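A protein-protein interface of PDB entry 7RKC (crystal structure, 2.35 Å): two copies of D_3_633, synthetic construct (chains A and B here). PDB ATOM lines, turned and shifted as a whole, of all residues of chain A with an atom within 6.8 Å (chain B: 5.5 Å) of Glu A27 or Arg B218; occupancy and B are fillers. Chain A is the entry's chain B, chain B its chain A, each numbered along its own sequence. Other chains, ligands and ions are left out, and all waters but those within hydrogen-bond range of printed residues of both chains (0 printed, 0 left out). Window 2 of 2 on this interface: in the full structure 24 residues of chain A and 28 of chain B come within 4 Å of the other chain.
NH2 of Arg B218 lies within salt-bridge range of OE2 of Glu A27, 2.5 Å away.
Leu B214 touches Leu A23 (CD1 to CG, 3.7 Å).
Ile B217 touches Leu A23 (CG2 to CD1, 3.5 Å).
Leu A23 touches Arg B218.
Leu B213 touches Leu A39 (CD2 to CB, 3.6 Å).
Leu A39 touches Leu B214 (CD1 to CB, 3.7 Å).
Leu A39 touches Ile B217 (O to CD1, 3.2 Å).
Leu A46 touches Ile B217.
Gln B220 touches Leu A46.
Of the printed residues of chain B, Glu A27 touches Arg B218 (2.5 Å).
Arg B218 touches just these residues of chain A: Leu A23 and Glu A27.
Of the printed residues of chain B, Leu A23 touches Leu B214 (3.7 Å), Ile B217 (3.5 Å) and Arg B218 (3.8 Å).
Printed residues of chain A within 4 Å of Leu B213: Leu A39 (3.6 Å).
Gln A25 touches none of the printed residues of chain B.
Leu B222 touches none of the printed residues of chain A.
The nearest residue of chain A that does not touch Arg B218 is Leu A46 (5.9 Å).
The nearest printed residue of chain A that does not touch Ile B217 is Leu A38 (6.2 Å).
Of the 13 printed residues of chain A, 4 touch a printed residue of chain B.
Printed residues of chain A that touch a printed residue of chain B: Leu A23, Glu A27, Leu A39 and Leu A46.
Hydrophobic or aromatic side chains of chain A that line the printed part of chain B: Leu A23, Leu A39 and Leu A46.
Along chain A the printed residues that touch a printed residue of chain B span positions 23 to 46.
Of the 11 printed residues of chain B, 5 touch a printed residue of chain A.
Among the printed residues, 9 pairs touch across the chains.
Among the printed residues, Asp or Glu carboxylates within 4 Å of a Lys or Arg side-chain nitrogen of the other chain: Glu A27 with Arg B218.
No position is printed for both chains.
Of the 9 pairs that touch across the chains among the printed residues, none has its exchanged pair printed and touching as well.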
ATOM      1  N   THR A  20      13.825  12.864  29.994  1.00  0.00           N
ATOM      2  CA  THR A  20      12.875  11.913  29.423  1.00  0.00           C
ATOM      3  C   THR A  20      12.180  12.496  28.198  1.00  0.00           C
ATOM      4  O   THR A  20      11.982  11.795  27.199  1.00  0.00           O
ATOM      5  CB  THR A  20      11.846  11.490  30.472  1.00  0.00           C
ATOM      6  OG1 THR A  20      11.257  12.653  31.069  1.00  0.00           O
ATOM      7  CG2 THR A  20      12.502  10.638  31.549  1.00  0.00           C
ATOM      8  N   LEU A  22      13.426  14.716  26.217  1.00  0.00           N
ATOM      9  CA  LEU A  22      14.429  14.704  25.159  1.00  0.00           C
ATOM     10  C   LEU A  22      14.625  13.298  24.605  1.00  0.00           C
ATOM     11  O   LEU A  22      14.834  13.123  23.399  1.00  0.00           O
ATOM     12  CB  LEU A  22      15.750  15.268  25.679  1.00  0.00           C
ATOM     13  CG  LEU A  22      15.862  16.794  25.717  1.00  0.00           C
ATOM     14  CD1 LEU A  22      16.993  17.228  26.634  1.00  0.00           C
ATOM     15  CD2 LEU A  22      16.056  17.355  24.317  1.00  0.00           C
ATOM     16  N   LEU A  23      14.569  12.286  25.475  1.00  0.00           N
ATOM     17  CA  LEU A  23      14.725  10.907  25.023  1.00  0.00           C
ATOM     18  C   LEU A  23      13.576  10.486  24.117  1.00  0.00           C
ATOM     19  O   LEU A  23      13.790   9.792  23.116  1.00  0.00           O
ATOM     20  CB  LEU A  23      14.826   9.971  26.225  1.00  0.00           C
ATOM     21  CG  LEU A  23      16.235   9.472  26.536  1.00  0.00           C
ATOM     22  CD1 LEU A  23      17.161  10.656  26.746  1.00  0.00           C
ATOM     23  CD2 LEU A  23      16.233   8.556  27.751  1.00  0.00           C
ATOM     24  N   GLU A  24      12.349  10.893  24.448  1.00  0.00           N
ATOM     25  CA  GLU A  24      11.214  10.543  23.604  1.00  0.00           C
ATOM     26  C   GLU A  24      11.292  11.232  22.248  1.00  0.00           C
ATOM     27  O   GLU A  24      10.786  10.700  21.253  1.00  0.00           O
ATOM     28  CB  GLU A  24       9.904  10.901  24.306  1.00  0.00           C
ATOM     29  N   GLN A  25      11.918  12.410  22.189  1.00  0.00           N
ATOM     30  CA  GLN A  25      12.099  13.086  20.909  1.00  0.00           C
ATOM     31  C   GLN A  25      13.139  12.380  20.047  1.00  0.00           C
ATOM     32  O   GLN A  25      12.987  12.301  18.822  1.00  0.00           O
ATOM     33  CB  GLN A  25      12.500  14.543  21.139  1.00  0.00           C
ATOM     34  CG  GLN A  25      11.353  15.453  21.540  1.00  0.00           C
ATOM     35  CD  GLN A  25      11.818  16.860  21.860  1.00  0.00           C
ATOM     36  OE1 GLN A  25      11.411  17.448  22.861  1.00  0.00           O
ATOM     37  NE2 GLN A  25      12.679  17.406  21.010  1.00  0.00           N
ATOM     38  N   ALA A  26      14.200  11.858  20.669  1.00  0.00           N
ATOM     39  CA  ALA A  26      15.248  11.189  19.905  1.00  0.00           C
ATOM     40  C   ALA A  26      14.774   9.862  19.329  1.00  0.00           C
ATOM     41  O   ALA A  26      15.289   9.419  18.296  1.00  0.00           O
ATOM     42  CB  ALA A  26      16.481  10.975  20.783  1.00  0.00           C
ATOM     43  N   GLU A  27      13.805   9.214  19.977  1.00  0.00           N
ATOM     44  CA  GLU A  27      13.312   7.935  19.475  1.00  0.00           C
ATOM     45  C   GLU A  27      12.482   8.120  18.212  1.00  0.00           C
ATOM     46  O   GLU A  27      12.605   7.340  17.260  1.00  0.00           O
ATOM     47  CB  GLU A  27      12.505   7.224  20.558  1.00  0.00           C
ATOM     48  CG  GLU A  27      13.316   6.900  21.798  1.00  0.00           C
ATOM     49  CD  GLU A  27      12.479   6.275  22.888  1.00  0.00           C
ATOM     50  OE1 GLU A  27      11.354   5.824  22.587  1.00  0.00           O
ATOM     51  OE2 GLU A  27      12.947   6.232  24.045  1.00  0.00           O
ATOM     52  N   ARG A  28      11.629   9.145  18.183  1.00  0.00           N
ATOM     53  CA  ARG A  28      10.763   9.422  17.045  1.00  0.00           C
ATOM     54  C   ARG A  28      11.361  10.467  16.109  1.00  0.00           C
ATOM     55  O   ARG A  28      10.623  11.225  15.470  1.00  0.00           O
ATOM     56  CB  ARG A  28       9.382   9.867  17.528  1.00  0.00           C
ATOM     57  N   ALA A  29      12.685  10.523  16.019  1.00  0.00           N
ATOM     58  CA  ALA A  29      13.355  11.480  15.145  1.00  0.00           C
ATOM     59  C   ALA A  29      13.748  10.829  13.823  1.00  0.00           C
ATOM     60  O   ALA A  29      14.631  11.315  13.117  1.00  0.00           O
ATOM     61  CB  ALA A  29      14.577  12.061  15.836  1.00  0.00           C
ATOM     62  N   ILE A  35      19.589  12.927  16.144  1.00  0.00           N
ATOM     63  CA  ILE A  35      19.306  12.050  17.274  1.00  0.00           C
ATOM     64  C   ILE A  35      20.448  12.094  18.281  1.00  0.00           C
ATOM     65  O   ILE A  35      20.221  12.079  19.497  1.00  0.00           O
ATOM     66  CB  ILE A  35      19.046  10.614  16.779  1.00  0.00           C
ATOM     67  CG1 ILE A  35      17.871  10.588  15.801  1.00  0.00           C
ATOM     68  CG2 ILE A  35      18.791   9.677  17.952  1.00  0.00           C
ATOM     69  N   LEU A  38      20.261  15.427  20.244  1.00  0.00           N
ATOM     70  CA  LEU A  38      19.244  15.466  21.286  1.00  0.00           C
ATOM     71  C   LEU A  38      19.600  14.604  22.489  1.00  0.00           C
ATOM     72  O   LEU A  38      19.072  14.843  23.581  1.00  0.00           O
ATOM     73  CB  LEU A  38      17.893  15.015  20.725  1.00  0.00           C
ATOM     74  CG  LEU A  38      17.163  15.994  19.803  1.00  0.00           C
ATOM     75  CD1 LEU A  38      16.158  15.254  18.935  1.00  0.00           C
ATOM     76  CD2 LEU A  38      16.480  17.084  20.611  1.00  0.00           C
ATOM     77  N   LEU A  39      20.480  13.617  22.322  1.00  0.00           N
ATOM     78  CA  LEU A  39      20.904  12.796  23.447  1.00  0.00           C
ATOM     79  C   LEU A  39      22.114  13.360  24.181  1.00  0.00           C
ATOM     80  O   LEU A  39      22.282  13.088  25.375  1.00  0.00           O
ATOM     81  CB  LEU A  39      21.210  11.372  22.975  1.00  0.00           C
ATOM     82  CG  LEU A  39      20.032  10.592  22.388  1.00  0.00           C
ATOM     83  CD1 LEU A  39      20.499   9.256  21.833  1.00  0.00           C
ATOM     84  CD2 LEU A  39      18.943  10.393  23.432  1.00  0.00           C
ATOM     85  N   LEU A  46      22.034  15.066  32.742  1.00  0.00           N
ATOM     86  CA  LEU A  46      22.320  14.054  33.754  1.00  0.00           C
ATOM     87  C   LEU A  46      23.603  14.379  34.506  1.00  0.00           C
ATOM     88  O   LEU A  46      23.690  14.168  35.722  1.00  0.00           O
ATOM     89  CB  LEU A  46      22.416  12.672  33.109  1.00  0.00           C
ATOM     90  CG  LEU A  46      21.168  12.133  32.406  1.00  0.00           C
ATOM     91  CD1 LEU A  46      21.468  10.788  31.761  1.00  0.00           C
ATOM     92  CD2 LEU A  46      20.000  12.022  33.379  1.00  0.00           C
ATOM     93  N   LEU B 199      21.419  -3.512  29.109  1.00  0.00           N
ATOM     94  CA  LEU B 199      21.619  -2.382  28.207  1.00  0.00           C
ATOM     95  C   LEU B 199      23.045  -2.331  27.678  1.00  0.00           C
ATOM     96  O   LEU B 199      23.277  -1.837  26.569  1.00  0.00           O
ATOM     97  CB  LEU B 199      21.270  -1.072  28.914  1.00  0.00           C
ATOM     98  CG  LEU B 199      19.781  -0.759  29.076  1.00  0.00           C
ATOM     99  CD1 LEU B 199      19.552   0.199  30.233  1.00  0.00           C
ATOM    100  CD2 LEU B 199      19.210  -0.191  27.787  1.00  0.00           C
ATOM    101  N   LEU B 213      24.378   5.395  22.841  1.00  0.00           N
ATOM    102  CA  LEU B 213      24.208   6.546  23.721  1.00  0.00           C
ATOM    103  C   LEU B 213      22.836   6.543  24.385  1.00  0.00           C
ATOM    104  O   LEU B 213      22.709   6.905  25.560  1.00  0.00           O
ATOM    105  CB  LEU B 213      24.424   7.838  22.933  1.00  0.00           C
ATOM    106  CG  LEU B 213      24.332   9.152  23.709  1.00  0.00           C
ATOM    107  CD1 LEU B 213      25.273   9.139  24.901  1.00  0.00           C
ATOM    108  CD2 LEU B 213      24.638  10.329  22.794  1.00  0.00           C
ATOM    109  N   LEU B 214      21.797   6.132  23.656  1.00  0.00           N
ATOM    110  CA  LEU B 214      20.457   6.147  24.231  1.00  0.00           C
ATOM    111  C   LEU B 214      20.290   5.056  25.280  1.00  0.00           C
ATOM    112  O   LEU B 214      19.576   5.249  26.269  1.00  0.00           O
ATOM    113  CB  LEU B 214      19.409   6.003  23.125  1.00  0.00           C
ATOM    114  CG  LEU B 214      17.981   5.631  23.532  1.00  0.00           C
ATOM    115  CD1 LEU B 214      17.336   6.766  24.312  1.00  0.00           C
ATOM    116  CD2 LEU B 214      17.144   5.277  22.313  1.00  0.00           C
ATOM    117  N   TYR B 215      20.957   3.915  25.097  1.00  0.00           N
ATOM    118  CA  TYR B 215      20.912   2.857  26.100  1.00  0.00           C
ATOM    119  C   TYR B 215      21.610   3.281  27.386  1.00  0.00           C
ATOM    120  O   TYR B 215      21.159   2.941  28.485  1.00  0.00           O
ATOM    121  CB  TYR B 215      21.542   1.581  25.541  1.00  0.00           C
ATOM    122  CG  TYR B 215      20.758   0.957  24.410  1.00  0.00           C
ATOM    123  CD1 TYR B 215      21.394   0.208  23.429  1.00  0.00           C
ATOM    124  CD2 TYR B 215      19.380   1.115  24.323  1.00  0.00           C
ATOM    125  CE1 TYR B 215      20.682  -0.365  22.393  1.00  0.00           C
ATOM    126  CE2 TYR B 215      18.659   0.545  23.293  1.00  0.00           C
ATOM    127  CZ  TYR B 215      19.315  -0.195  22.330  1.00  0.00           C
ATOM    128  OH  TYR B 215      18.602  -0.764  21.299  1.00  0.00           O
ATOM    129  N   VAL B 216      22.707   4.033  27.271  1.00  0.00           N
ATOM    130  CA  VAL B 216      23.446   4.442  28.461  1.00  0.00           C
ATOM    131  C   VAL B 216      22.703   5.546  29.202  1.00  0.00           C
ATOM    132  O   VAL B 216      22.696   5.588  30.437  1.00  0.00           O
ATOM    133  CB  VAL B 216      24.874   4.876  28.077  1.00  0.00           C
ATOM    134  CG1 VAL B 216      25.627   5.382  29.299  1.00  0.00           C
ATOM    135  CG2 VAL B 216      25.621   3.720  27.432  1.00  0.00           C
ATOM    136  N   ILE B 217      22.048   6.446  28.465  1.00  0.00           N
ATOM    137  CA  ILE B 217      21.249   7.479  29.115  1.00  0.00           C
ATOM    138  C   ILE B 217      20.038   6.859  29.802  1.00  0.00           C
ATOM    139  O   ILE B 217      19.634   7.291  30.890  1.00  0.00           O
ATOM    140  CB  ILE B 217      20.844   8.561  28.100  1.00  0.00           C
ATOM    141  CG1 ILE B 217      22.080   9.339  27.646  1.00  0.00           C
ATOM    142  CG2 ILE B 217      19.841   9.513  28.712  1.00  0.00           C
ATOM    143  CD1 ILE B 217      21.878  10.104  26.367  1.00  0.00           C
ATOM    144  N   ARG B 218      19.455   5.821  29.195  1.00  0.00           N
ATOM    145  CA  ARG B 218      18.354   5.117  29.840  1.00  0.00           C
ATOM    146  C   ARG B 218      18.817   4.336  31.059  1.00  0.00           C
ATOM    147  O   ARG B 218      18.006   4.058  31.949  1.00  0.00           O
ATOM    148  CB  ARG B 218      17.689   4.152  28.859  1.00  0.00           C
ATOM    149  CG  ARG B 218      16.708   4.775  27.889  1.00  0.00           C
ATOM    150  CD  ARG B 218      16.235   3.716  26.908  1.00  0.00           C
ATOM    151  NE  ARG B 218      15.103   4.153  26.100  1.00  0.00           N
ATOM    152  CZ  ARG B 218      14.544   3.410  25.151  1.00  0.00           C
ATOM    153  NH1 ARG B 218      15.023   2.202  24.885  1.00  0.00           N
ATOM    154  NH2 ARG B 218      13.516   3.876  24.460  1.00  0.00           N
ATOM    155  N   ALA B 219      20.104   3.991  31.127  1.00  0.00           N
ATOM    156  CA  ALA B 219      20.630   3.308  32.301  1.00  0.00           C
ATOM    157  C   ALA B 219      20.991   4.297  33.399  1.00  0.00           C
ATOM    158  O   ALA B 219      20.787   4.013  34.585  1.00  0.00           O
ATOM    159  CB  ALA B 219      21.849   2.468  31.920  1.00  0.00           C
ATOM    160  N   GLN B 220      21.527   5.463  33.026  1.00  0.00           N
ATOM    161  CA  GLN B 220      21.851   6.467  34.030  1.00  0.00           C
ATOM    162  C   GLN B 220      20.594   7.070  34.639  1.00  0.00           C
ATOM    163  O   GLN B 220      20.595   7.439  35.819  1.00  0.00           O
ATOM    164  CB  GLN B 220      22.736   7.556  33.423  1.00  0.00           C
ATOM    165  CG  GLN B 220      24.072   7.048  32.892  1.00  0.00           C
ATOM    166  CD  GLN B 220      25.074   6.727  33.990  1.00  0.00           C
ATOM    167  OE1 GLN B 220      24.712   6.534  35.151  1.00  0.00           O
ATOM    168  NE2 GLN B 220      26.347   6.663  33.620  1.00  0.00           N
ATOM    169  N   LEU B 221      19.517   7.176  33.857  1.00  0.00           N
ATOM    170  CA  LEU B 221      18.258   7.672  34.401  1.00  0.00           C
ATOM    171  C   LEU B 221      17.733   6.742  35.487  1.00  0.00           C
ATOM    172  O   LEU B 221      17.203   7.199  36.507  1.00  0.00           O
ATOM    173  CB  LEU B 221      17.228   7.835  33.282  1.00  0.00           C
ATOM    174  CG  LEU B 221      16.409   9.128  33.295  1.00  0.00           C
ATOM    175  N   LEU B 222      17.877   5.429  35.287  1.00  0.00           N
ATOM    176  CA  LEU B 222      17.450   4.471  36.299  1.00  0.00           C
ATOM    177  C   LEU B 222      18.409   4.438  37.482  1.00  0.00           C
ATOM    178  O   LEU B 222      17.983   4.202  38.618  1.00  0.00           O
ATOM    179  CB  LEU B 222      17.330   3.073  35.690  1.00  0.00           C
ATOM    180  CG  LEU B 222      16.281   2.854  34.598  1.00  0.00           C
ATOM    181  CD1 LEU B 222      16.616   1.611  33.789  1.00  0.00           C
ATOM    182  CD2 LEU B 222      14.894   2.740  35.206  1.00  0.00           C
